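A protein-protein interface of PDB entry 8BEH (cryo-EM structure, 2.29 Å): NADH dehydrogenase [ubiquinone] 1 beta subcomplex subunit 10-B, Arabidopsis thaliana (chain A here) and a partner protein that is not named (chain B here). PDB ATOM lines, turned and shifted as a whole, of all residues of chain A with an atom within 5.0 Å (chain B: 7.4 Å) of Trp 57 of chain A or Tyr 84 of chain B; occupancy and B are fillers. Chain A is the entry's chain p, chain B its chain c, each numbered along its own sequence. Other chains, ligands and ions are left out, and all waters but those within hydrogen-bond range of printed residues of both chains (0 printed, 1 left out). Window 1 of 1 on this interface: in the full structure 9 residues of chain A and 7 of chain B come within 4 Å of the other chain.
The backbone carbonyl oxygen (O) of Glu 87 of chain B sits at hydrogen-bond distance from the side-chain amino group (NZ) of Lys 54 of chain A, at 2.9 Å.
NZ of Lys 54 of chain A lies within hydrogen-bond range of O of Glu 85 of chain B (2.6 Å).
The side-chain sulfur (SG) of Cys 58 of chain A lies close to the side-chain hydroxyl (OH) of Tyr 84 of chain B, at 3.6 Å.
NE1 of Trp 57 of chain A lies close to OE2 of Glu 87 of chain B (3.4 Å).
The side-chain carboxylate (OE2) of Glu 62 of chain A sits at hydrogen-bond distance from the side-chain hydroxyl (OH) of Tyr 84 of chain B (2.6 Å).
The side-chain carboxylate of Glu 53 of chain A is in salt-bridge range of the side-chain amino group of Lys 56 of chain A, 2.9 Å away.
SG of Cys 58 of chain A lies close to O of Lys 69 of chain A.
NZ of Lys 81 of chain B lies within salt-bridge range of OE2 of Glu 87 of chain B (3.3 Å).
Among the printed residues, pairs that only touch across the chains: Leu 73 of chain A with Glu 85 of chain B (3.1 Å), Glu 53 of chain A with His 88 of chain B (3.2 Å), Val 61 of chain A with Lys 81 of chain B (3.2 Å), Trp 57 of chain A with Lys 81 of chain B (3.5 Å), Lys 54 of chain A with Tyr 84 of chain B (3.5 Å), Trp 57 of chain A with Tyr 84 of chain B (3.6 Å), Trp 57 of chain A with Pro 62 of chain B (3.9 Å), Val 61 of chain A with Pro 62 of chain B (3.9 Å), Leu 73 of chain A with Tyr 84 of chain B (3.96 Å) and Val 61 of chain A with Tyr 84 of chain B (3.97 Å).
Trp 57 of chain A touches four residues of chain B.
Printed residues of chain B within 4 Å of Leu 73 of chain A: Tyr 84 and Glu 85.
Tyr 84 of chain B touches six residues of chain A.
Printed residues of chain A within 4 Å of His 88 of chain B: Glu 53.
The nearest residue of chain B that does not touch Trp 57 of chain A is Gln 60 of chain B (4.1 Å).
Hydrophobic or aromatic side chains of chain B that line the printed part of chain A: Pro 62 and Tyr 84.
Of the 12 printed residues of chain A, 7 touch a printed residue of chain B.
Hydrophobic or aromatic side chains of chain A within 4 Å of the printed part of chain B: Trp 57, Val 61 and Leu 73.
Among the printed residues, no Asp or Glu carboxylate lies within 4 Å of a Lys or Arg side-chain nitrogen of the other chain.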
ATOM      1  N   GLU A  53      10.497  -1.708  -2.980  1.00  0.00           N
ATOM      2  CA  GLU A  53      11.225  -1.567  -4.278  1.00  0.00           C
ATOM      3  C   GLU A  53      12.491  -0.656  -4.102  1.00  0.00           C
ATOM      4  O   GLU A  53      13.517  -1.107  -4.524  1.00  0.00           O
ATOM      5  CB  GLU A  53      10.239  -1.163  -5.384  1.00  0.00           C
ATOM      6  CG  GLU A  53      10.407  -1.968  -6.634  1.00  0.00           C
ATOM      7  CD  GLU A  53      10.292  -3.461  -6.406  1.00  0.00           C
ATOM      8  OE1 GLU A  53       9.418  -3.873  -5.635  1.00  0.00           O
ATOM      9  OE2 GLU A  53      11.095  -4.197  -6.984  1.00  0.00           O
ATOM     10  N   LYS A  54      12.394   0.444  -3.344  1.00  0.00           N
ATOM     11  CA  LYS A  54      13.570   1.341  -3.003  1.00  0.00           C
ATOM     12  C   LYS A  54      14.688   0.587  -2.278  1.00  0.00           C
ATOM     13  O   LYS A  54      15.744   0.573  -2.803  1.00  0.00           O
ATOM     14  CB  LYS A  54      13.066   2.600  -2.285  1.00  0.00           C
ATOM     15  CG  LYS A  54      12.098   3.449  -3.100  1.00  0.00           C
ATOM     16  CD  LYS A  54      11.712   4.743  -2.423  1.00  0.00           C
ATOM     17  CE  LYS A  54      10.383   5.321  -2.854  1.00  0.00           C
ATOM     18  NZ  LYS A  54      10.245   5.465  -4.320  1.00  0.00           N
ATOM     19  N   VAL A  55      14.342  -0.166  -1.231  1.00  0.00           N
ATOM     20  CA  VAL A  55      15.292  -0.986  -0.456  1.00  0.00           C
ATOM     21  C   VAL A  55      15.900  -2.019  -1.369  1.00  0.00           C
ATOM     22  O   VAL A  55      17.110  -2.059  -1.360  1.00  0.00           O
ATOM     23  CB  VAL A  55      14.658  -1.568   0.832  1.00  0.00           C
ATOM     24  CG1 VAL A  55      15.548  -2.546   1.555  1.00  0.00           C
ATOM     25  CG2 VAL A  55      14.164  -0.473   1.758  1.00  0.00           C
ATOM     26  N   LYS A  56      15.069  -2.758  -2.119  1.00  0.00           N
ATOM     27  CA  LYS A  56      15.525  -3.815  -3.008  1.00  0.00           C
ATOM     28  C   LYS A  56      16.681  -3.237  -3.862  1.00  0.00           C
ATOM     29  O   LYS A  56      17.765  -3.770  -3.780  1.00  0.00           O
ATOM     30  CB  LYS A  56      14.370  -4.376  -3.862  1.00  0.00           C
ATOM     31  CG  LYS A  56      14.666  -5.554  -4.767  1.00  0.00           C
ATOM     32  CD  LYS A  56      13.485  -5.987  -5.614  1.00  0.00           C
ATOM     33  CE  LYS A  56      12.364  -6.659  -4.848  1.00  0.00           C
ATOM     34  NZ  LYS A  56      11.286  -5.735  -4.420  1.00  0.00           N
ATOM     35  N   TRP A  57      16.405  -2.152  -4.541  1.00  0.00           N
ATOM     36  CA  TRP A  57      17.366  -1.526  -5.482  1.00  0.00           C
ATOM     37  C   TRP A  57      18.571  -0.882  -4.803  1.00  0.00           C
ATOM     38  O   TRP A  57      19.600  -1.070  -5.349  1.00  0.00           O
ATOM     39  CB  TRP A  57      16.621  -0.632  -6.462  1.00  0.00           C
ATOM     40  CG  TRP A  57      15.913  -1.524  -7.433  1.00  0.00           C
ATOM     41  CD1 TRP A  57      14.568  -1.727  -7.537  1.00  0.00           C
ATOM     42  CD2 TRP A  57      16.525  -2.441  -8.357  1.00  0.00           C
ATOM     43  NE1 TRP A  57      14.306  -2.665  -8.491  1.00  0.00           N
ATOM     44  CE2 TRP A  57      15.480  -3.117  -9.021  1.00  0.00           C
ATOM     45  CE3 TRP A  57      17.847  -2.736  -8.710  1.00  0.00           C
ATOM     46  CZ2 TRP A  57      15.714  -4.074 -10.005  1.00  0.00           C
ATOM     47  CZ3 TRP A  57      18.077  -3.679  -9.683  1.00  0.00           C
ATOM     48  CH2 TRP A  57      17.025  -4.331 -10.332  1.00  0.00           C
ATOM     49  N   CYS A  58      18.414  -0.273  -3.630  1.00  0.00           N
ATOM     50  CA  CYS A  58      19.559   0.309  -2.884  1.00  0.00           C
ATOM     51  C   CYS A  58      20.512  -0.824  -2.471  1.00  0.00           C
ATOM     52  O   CYS A  58      21.645  -0.716  -2.850  1.00  0.00           O
ATOM     53  CB  CYS A  58      19.062   1.249  -1.791  1.00  0.00           C
ATOM     54  SG  CYS A  58      20.337   2.064  -0.804  1.00  0.00           S
ATOM     55  N   TYR A  59      20.027  -1.910  -1.856  1.00  0.00           N
ATOM     56  CA  TYR A  59      20.819  -3.116  -1.574  1.00  0.00           C
ATOM     57  C   TYR A  59      21.592  -3.506  -2.827  1.00  0.00           C
ATOM     58  O   TYR A  59      22.778  -3.635  -2.680  1.00  0.00           O
ATOM     59  CB  TYR A  59      20.002  -4.284  -0.984  1.00  0.00           C
ATOM     60  CG  TYR A  59      20.768  -5.465  -0.485  1.00  0.00           C
ATOM     61  CD1 TYR A  59      21.224  -5.496   0.819  1.00  0.00           C
ATOM     62  CD2 TYR A  59      21.006  -6.552  -1.306  1.00  0.00           C
ATOM     63  CE1 TYR A  59      21.909  -6.583   1.300  1.00  0.00           C
ATOM     64  CE2 TYR A  59      21.691  -7.654  -0.836  1.00  0.00           C
ATOM     65  CZ  TYR A  59      22.144  -7.660   0.469  1.00  0.00           C
ATOM     66  OH  TYR A  59      22.823  -8.713   0.974  1.00  0.00           O
ATOM     67  N   ARG A  60      20.910  -3.696  -3.943  1.00  0.00           N
ATOM     68  CA  ARG A  60      21.485  -4.136  -5.212  1.00  0.00           C
ATOM     69  C   ARG A  60      22.477  -3.109  -5.767  1.00  0.00           C
ATOM     70  O   ARG A  60      23.426  -3.500  -6.352  1.00  0.00           O
ATOM     71  CB  ARG A  60      20.362  -4.403  -6.222  1.00  0.00           C
ATOM     72  CG  ARG A  60      19.559  -5.662  -5.929  1.00  0.00           C
ATOM     73  CD  ARG A  60      18.274  -5.819  -6.701  1.00  0.00           C
ATOM     74  NE  ARG A  60      17.604  -7.046  -6.306  1.00  0.00           N
ATOM     75  CZ  ARG A  60      16.601  -7.611  -6.961  1.00  0.00           C
ATOM     76  NH1 ARG A  60      16.115  -7.063  -8.055  1.00  0.00           N
ATOM     77  NH2 ARG A  60      16.088  -8.731  -6.507  1.00  0.00           N
ATOM     78  N   VAL A  61      22.130  -1.844  -5.656  1.00  0.00           N
ATOM     79  CA  VAL A  61      23.042  -0.893  -6.280  1.00  0.00           C
ATOM     80  C   VAL A  61      24.248  -0.620  -5.387  1.00  0.00           C
ATOM     81  O   VAL A  61      25.379  -0.526  -5.868  1.00  0.00           O
ATOM     82  CB  VAL A  61      22.287   0.399  -6.648  1.00  0.00           C
ATOM     83  CG1 VAL A  61      23.246   1.567  -6.829  1.00  0.00           C
ATOM     84  CG2 VAL A  61      21.464   0.191  -7.912  1.00  0.00           C
ATOM     85  N   GLU A  62      24.043  -0.513  -4.077  1.00  0.00           N
ATOM     86  CA  GLU A  62      25.106  -0.072  -3.184  1.00  0.00           C
ATOM     87  C   GLU A  62      25.994  -1.194  -2.662  1.00  0.00           C
ATOM     88  O   GLU A  62      27.054  -0.901  -2.102  1.00  0.00           O
ATOM     89  CB  GLU A  62      24.511   0.699  -2.005  1.00  0.00           C
ATOM     90  CG  GLU A  62      23.627   1.852  -2.424  1.00  0.00           C
ATOM     91  CD  GLU A  62      24.404   3.045  -2.956  1.00  0.00           C
ATOM     92  OE1 GLU A  62      25.617   2.925  -3.203  1.00  0.00           O
ATOM     93  OE2 GLU A  62      23.792   4.113  -3.133  1.00  0.00           O
ATOM     94  N   LYS A  69      24.036   3.325   3.167  1.00  0.00           N
ATOM     95  CA  LYS A  69      23.254   3.999   2.137  1.00  0.00           C
ATOM     96  C   LYS A  69      21.753   3.726   2.225  1.00  0.00           C
ATOM     97  O   LYS A  69      20.963   4.620   1.912  1.00  0.00           O
ATOM     98  CB  LYS A  69      23.762   3.612   0.746  1.00  0.00           C
ATOM     99  CG  LYS A  69      25.212   3.997   0.490  1.00  0.00           C
ATOM    100  CD  LYS A  69      25.395   5.502   0.516  1.00  0.00           C
ATOM    101  CE  LYS A  69      26.820   5.917   0.190  1.00  0.00           C
ATOM    102  NZ  LYS A  69      27.013   7.393   0.237  1.00  0.00           N
ATOM    103  N   LEU A  73      15.995   4.500   3.935  1.00  0.00           N
ATOM    104  CA  LEU A  73      14.978   3.729   3.225  1.00  0.00           C
ATOM    105  C   LEU A  73      14.526   2.531   4.047  1.00  0.00           C
ATOM    106  O   LEU A  73      13.333   2.212   4.082  1.00  0.00           O
ATOM    107  CB  LEU A  73      15.508   3.281   1.866  1.00  0.00           C
ATOM    108  CG  LEU A  73      15.601   4.358   0.787  1.00  0.00           C
ATOM    109  CD1 LEU A  73      16.080   3.767  -0.526  1.00  0.00           C
ATOM    110  CD2 LEU A  73      14.267   5.070   0.611  1.00  0.00           C
ATOM    111  N   GLN B  60      18.657  -7.061 -15.857  1.00  0.00           N
ATOM    112  CA  GLN B  60      18.966  -5.777 -15.239  1.00  0.00           C
ATOM    113  C   GLN B  60      20.371  -5.848 -14.659  1.00  0.00           C
ATOM    114  O   GLN B  60      20.639  -6.669 -13.775  1.00  0.00           O
ATOM    115  CB  GLN B  60      17.953  -5.420 -14.146  1.00  0.00           C
ATOM    116  CG  GLN B  60      16.513  -5.316 -14.625  1.00  0.00           C
ATOM    117  CD  GLN B  60      16.254  -4.103 -15.494  1.00  0.00           C
ATOM    118  OE1 GLN B  60      16.765  -3.019 -15.236  1.00  0.00           O
ATOM    119  NE2 GLN B  60      15.461  -4.287 -16.538  1.00  0.00           N
ATOM    120  N   ARG B  61      21.262  -4.989 -15.150  1.00  0.00           N
ATOM    121  CA  ARG B  61      22.661  -4.954 -14.721  1.00  0.00           C
ATOM    122  C   ARG B  61      22.955  -3.585 -14.124  1.00  0.00           C
ATOM    123  O   ARG B  61      23.322  -2.648 -14.846  1.00  0.00           O
ATOM    124  CB  ARG B  61      23.601  -5.264 -15.885  1.00  0.00           C
ATOM    125  CG  ARG B  61      23.111  -6.353 -16.829  1.00  0.00           C
ATOM    126  CD  ARG B  61      22.987  -7.697 -16.124  1.00  0.00           C
ATOM    127  NE  ARG B  61      24.284  -8.260 -15.770  1.00  0.00           N
ATOM    128  CZ  ARG B  61      25.086  -8.898 -16.612  1.00  0.00           C
ATOM    129  NH1 ARG B  61      24.753  -9.087 -17.875  1.00  0.00           N
ATOM    130  NH2 ARG B  61      26.252  -9.356 -16.171  1.00  0.00           N
ATOM    131  N   PRO B  62      22.795  -3.423 -12.809  1.00  0.00           N
ATOM    132  CA  PRO B  62      23.018  -2.100 -12.204  1.00  0.00           C
ATOM    133  C   PRO B  62      24.452  -1.609 -12.300  1.00  0.00           C
ATOM    134  O   PRO B  62      24.686  -0.400 -12.200  1.00  0.00           O
ATOM    135  CB  PRO B  62      22.603  -2.311 -10.742  1.00  0.00           C
ATOM    136  CG  PRO B  62      21.803  -3.569 -10.734  1.00  0.00           C
ATOM    137  CD  PRO B  62      22.359  -4.416 -11.816  1.00  0.00           C
ATOM    138  N   THR B  80      21.133   1.476 -15.025  1.00  0.00           N
ATOM    139  CA  THR B  80      19.831   2.121 -15.100  1.00  0.00           C
ATOM    140  C   THR B  80      19.158   2.274 -13.740  1.00  0.00           C
ATOM    141  O   THR B  80      18.239   3.087 -13.607  1.00  0.00           O
ATOM    142  CB  THR B  80      18.917   1.333 -16.056  1.00  0.00           C
ATOM    143  OG1 THR B  80      19.547   1.238 -17.336  1.00  0.00           O
ATOM    144  CG2 THR B  80      17.564   2.018 -16.249  1.00  0.00           C
ATOM    145  N   LYS B  81      19.618   1.554 -12.722  1.00  0.00           N
ATOM    146  CA  LYS B  81      18.992   1.569 -11.409  1.00  0.00           C
ATOM    147  C   LYS B  81      19.663   2.530 -10.435  1.00  0.00           C
ATOM    148  O   LYS B  81      19.474   2.393  -9.222  1.00  0.00           O
ATOM    149  CB  LYS B  81      18.978   0.157 -10.823  1.00  0.00           C
ATOM    150  CG  LYS B  81      18.189  -0.839 -11.645  1.00  0.00           C
ATOM    151  CD  LYS B  81      16.773  -0.368 -11.866  1.00  0.00           C
ATOM    152  CE  LYS B  81      15.929  -1.456 -12.503  1.00  0.00           C
ATOM    153  NZ  LYS B  81      14.481  -1.218 -12.322  1.00  0.00           N
ATOM    154  N   ASP B  82      20.424   3.506 -10.931  1.00  0.00           N
ATOM    155  CA  ASP B  82      21.185   4.374 -10.038  1.00  0.00           C
ATOM    156  C   ASP B  82      20.275   5.208  -9.150  1.00  0.00           C
ATOM    157  O   ASP B  82      20.593   5.455  -7.982  1.00  0.00           O
ATOM    158  CB  ASP B  82      22.112   5.276 -10.845  1.00  0.00           C
ATOM    159  CG  ASP B  82      23.397   4.587 -11.210  1.00  0.00           C
ATOM    160  OD1 ASP B  82      23.845   3.737 -10.420  1.00  0.00           O
ATOM    161  OD2 ASP B  82      23.954   4.884 -12.285  1.00  0.00           O
ATOM    162  N   ASP B  83      19.148   5.661  -9.688  1.00  0.00           N
ATOM    163  CA  ASP B  83      18.204   6.469  -8.924  1.00  0.00           C
ATOM    164  C   ASP B  83      17.132   5.560  -8.323  1.00  0.00           C
ATOM    165  O   ASP B  83      15.963   5.561  -8.712  1.00  0.00           O
ATOM    166  CB  ASP B  83      17.610   7.556  -9.809  1.00  0.00           C
ATOM    167  CG  ASP B  83      16.926   8.634  -9.016  1.00  0.00           C
ATOM    168  OD1 ASP B  83      16.945   8.563  -7.770  1.00  0.00           O
ATOM    169  OD2 ASP B  83      16.386   9.573  -9.637  1.00  0.00           O
ATOM    170  N   TYR B  84      17.563   4.768  -7.341  1.00  0.00           N
ATOM    171  CA  TYR B  84      16.661   3.825  -6.694  1.00  0.00           C
ATOM    172  C   TYR B  84      15.618   4.513  -5.827  1.00  0.00           C
ATOM    173  O   TYR B  84      14.656   3.862  -5.409  1.00  0.00           O
ATOM    174  CB  TYR B  84      17.462   2.812  -5.869  1.00  0.00           C
ATOM    175  CG  TYR B  84      18.528   3.403  -4.978  1.00  0.00           C
ATOM    176  CD1 TYR B  84      18.191   4.151  -3.859  1.00  0.00           C
ATOM    177  CD2 TYR B  84      19.876   3.234  -5.271  1.00  0.00           C
ATOM    178  CE1 TYR B  84      19.156   4.691  -3.050  1.00  0.00           C
ATOM    179  CE2 TYR B  84      20.852   3.775  -4.465  1.00  0.00           C
ATOM    180  CZ  TYR B  84      20.488   4.502  -3.357  1.00  0.00           C
ATOM    181  OH  TYR B  84      21.455   5.041  -2.547  1.00  0.00           O
ATOM    182  N   GLU B  85      15.781   5.809  -5.559  1.00  0.00           N
ATOM    183  CA  GLU B  85      14.780   6.552  -4.807  1.00  0.00           C
ATOM    184  C   GLU B  85      13.466   6.669  -5.569  1.00  0.00           C
ATOM    185  O   GLU B  85      12.409   6.813  -4.952  1.00  0.00           O
ATOM    186  CB  GLU B  85      15.314   7.941  -4.471  1.00  0.00           C
ATOM    187  CG  GLU B  85      15.169   8.351  -3.024  1.00  0.00           C
ATOM    188  CD  GLU B  85      15.984   7.496  -2.086  1.00  0.00           C
ATOM    189  OE1 GLU B  85      17.000   6.927  -2.528  1.00  0.00           O
ATOM    190  OE2 GLU B  85      15.625   7.415  -0.895  1.00  0.00           O
ATOM    191  N   LYS B  86      13.538   6.682  -6.875  1.00  0.00           N
ATOM    192  CA  LYS B  86      12.352   6.767  -7.743  1.00  0.00           C
ATOM    193  C   LYS B  86      11.779   5.378  -8.101  1.00  0.00           C
ATOM    194  O   LYS B  86      10.844   5.317  -8.839  1.00  0.00           O
ATOM    195  CB  LYS B  86      12.863   7.619  -8.909  1.00  0.00           C
ATOM    196  CG  LYS B  86      13.540   8.925  -8.546  1.00  0.00           C
ATOM    197  CD  LYS B  86      12.625  10.009  -8.062  1.00  0.00           C
ATOM    198  CE  LYS B  86      13.167  11.385  -8.380  1.00  0.00           C
ATOM    199  NZ  LYS B  86      13.534  11.496  -9.810  1.00  0.00           N
ATOM    200  N   GLU B  87      12.371   4.297  -7.636  1.00  0.00           N
ATOM    201  CA  GLU B  87      11.791   2.946  -7.869  1.00  0.00           C
ATOM    202  C   GLU B  87      10.336   2.841  -7.376  1.00  0.00           C
ATOM    203  O   GLU B  87      10.016   3.442  -6.352  1.00  0.00           O
ATOM    204  CB  GLU B  87      12.656   1.869  -7.239  1.00  0.00           C
ATOM    205  CG  GLU B  87      13.918   1.601  -8.014  1.00  0.00           C
ATOM    206  CD  GLU B  87      13.642   1.288  -9.462  1.00  0.00           C
ATOM    207  OE1 GLU B  87      13.946   2.136 -10.300  1.00  0.00           O
ATOM    208  OE2 GLU B  87      13.092   0.212  -9.738  1.00  0.00           O
ATOM    209  N   HIS B  88       9.494   2.142  -8.115  1.00  0.00           N
ATOM    210  CA  HIS B  88       8.076   1.901  -7.691  1.00  0.00           C
ATOM    211  C   HIS B  88       7.602   0.501  -8.098  1.00  0.00           C
ATOM    212  O   HIS B  88       8.440  -0.261  -8.514  1.00  0.00           O
ATOM    213  CB  HIS B  88       7.175   3.031  -8.129  1.00  0.00           C
ATOM    214  CG  HIS B  88       6.942   3.174  -9.584  1.00  0.00           C
ATOM    215  ND1 HIS B  88       5.956   2.475 -10.235  1.00  0.00           N
ATOM    216  CD2 HIS B  88       7.490   4.000 -10.486  1.00  0.00           C
ATOM    217  CE1 HIS B  88       5.952   2.825 -11.496  1.00  0.00           C
ATOM    218  NE2 HIS B  88       6.872   3.760 -11.668  1.00  0.00           N
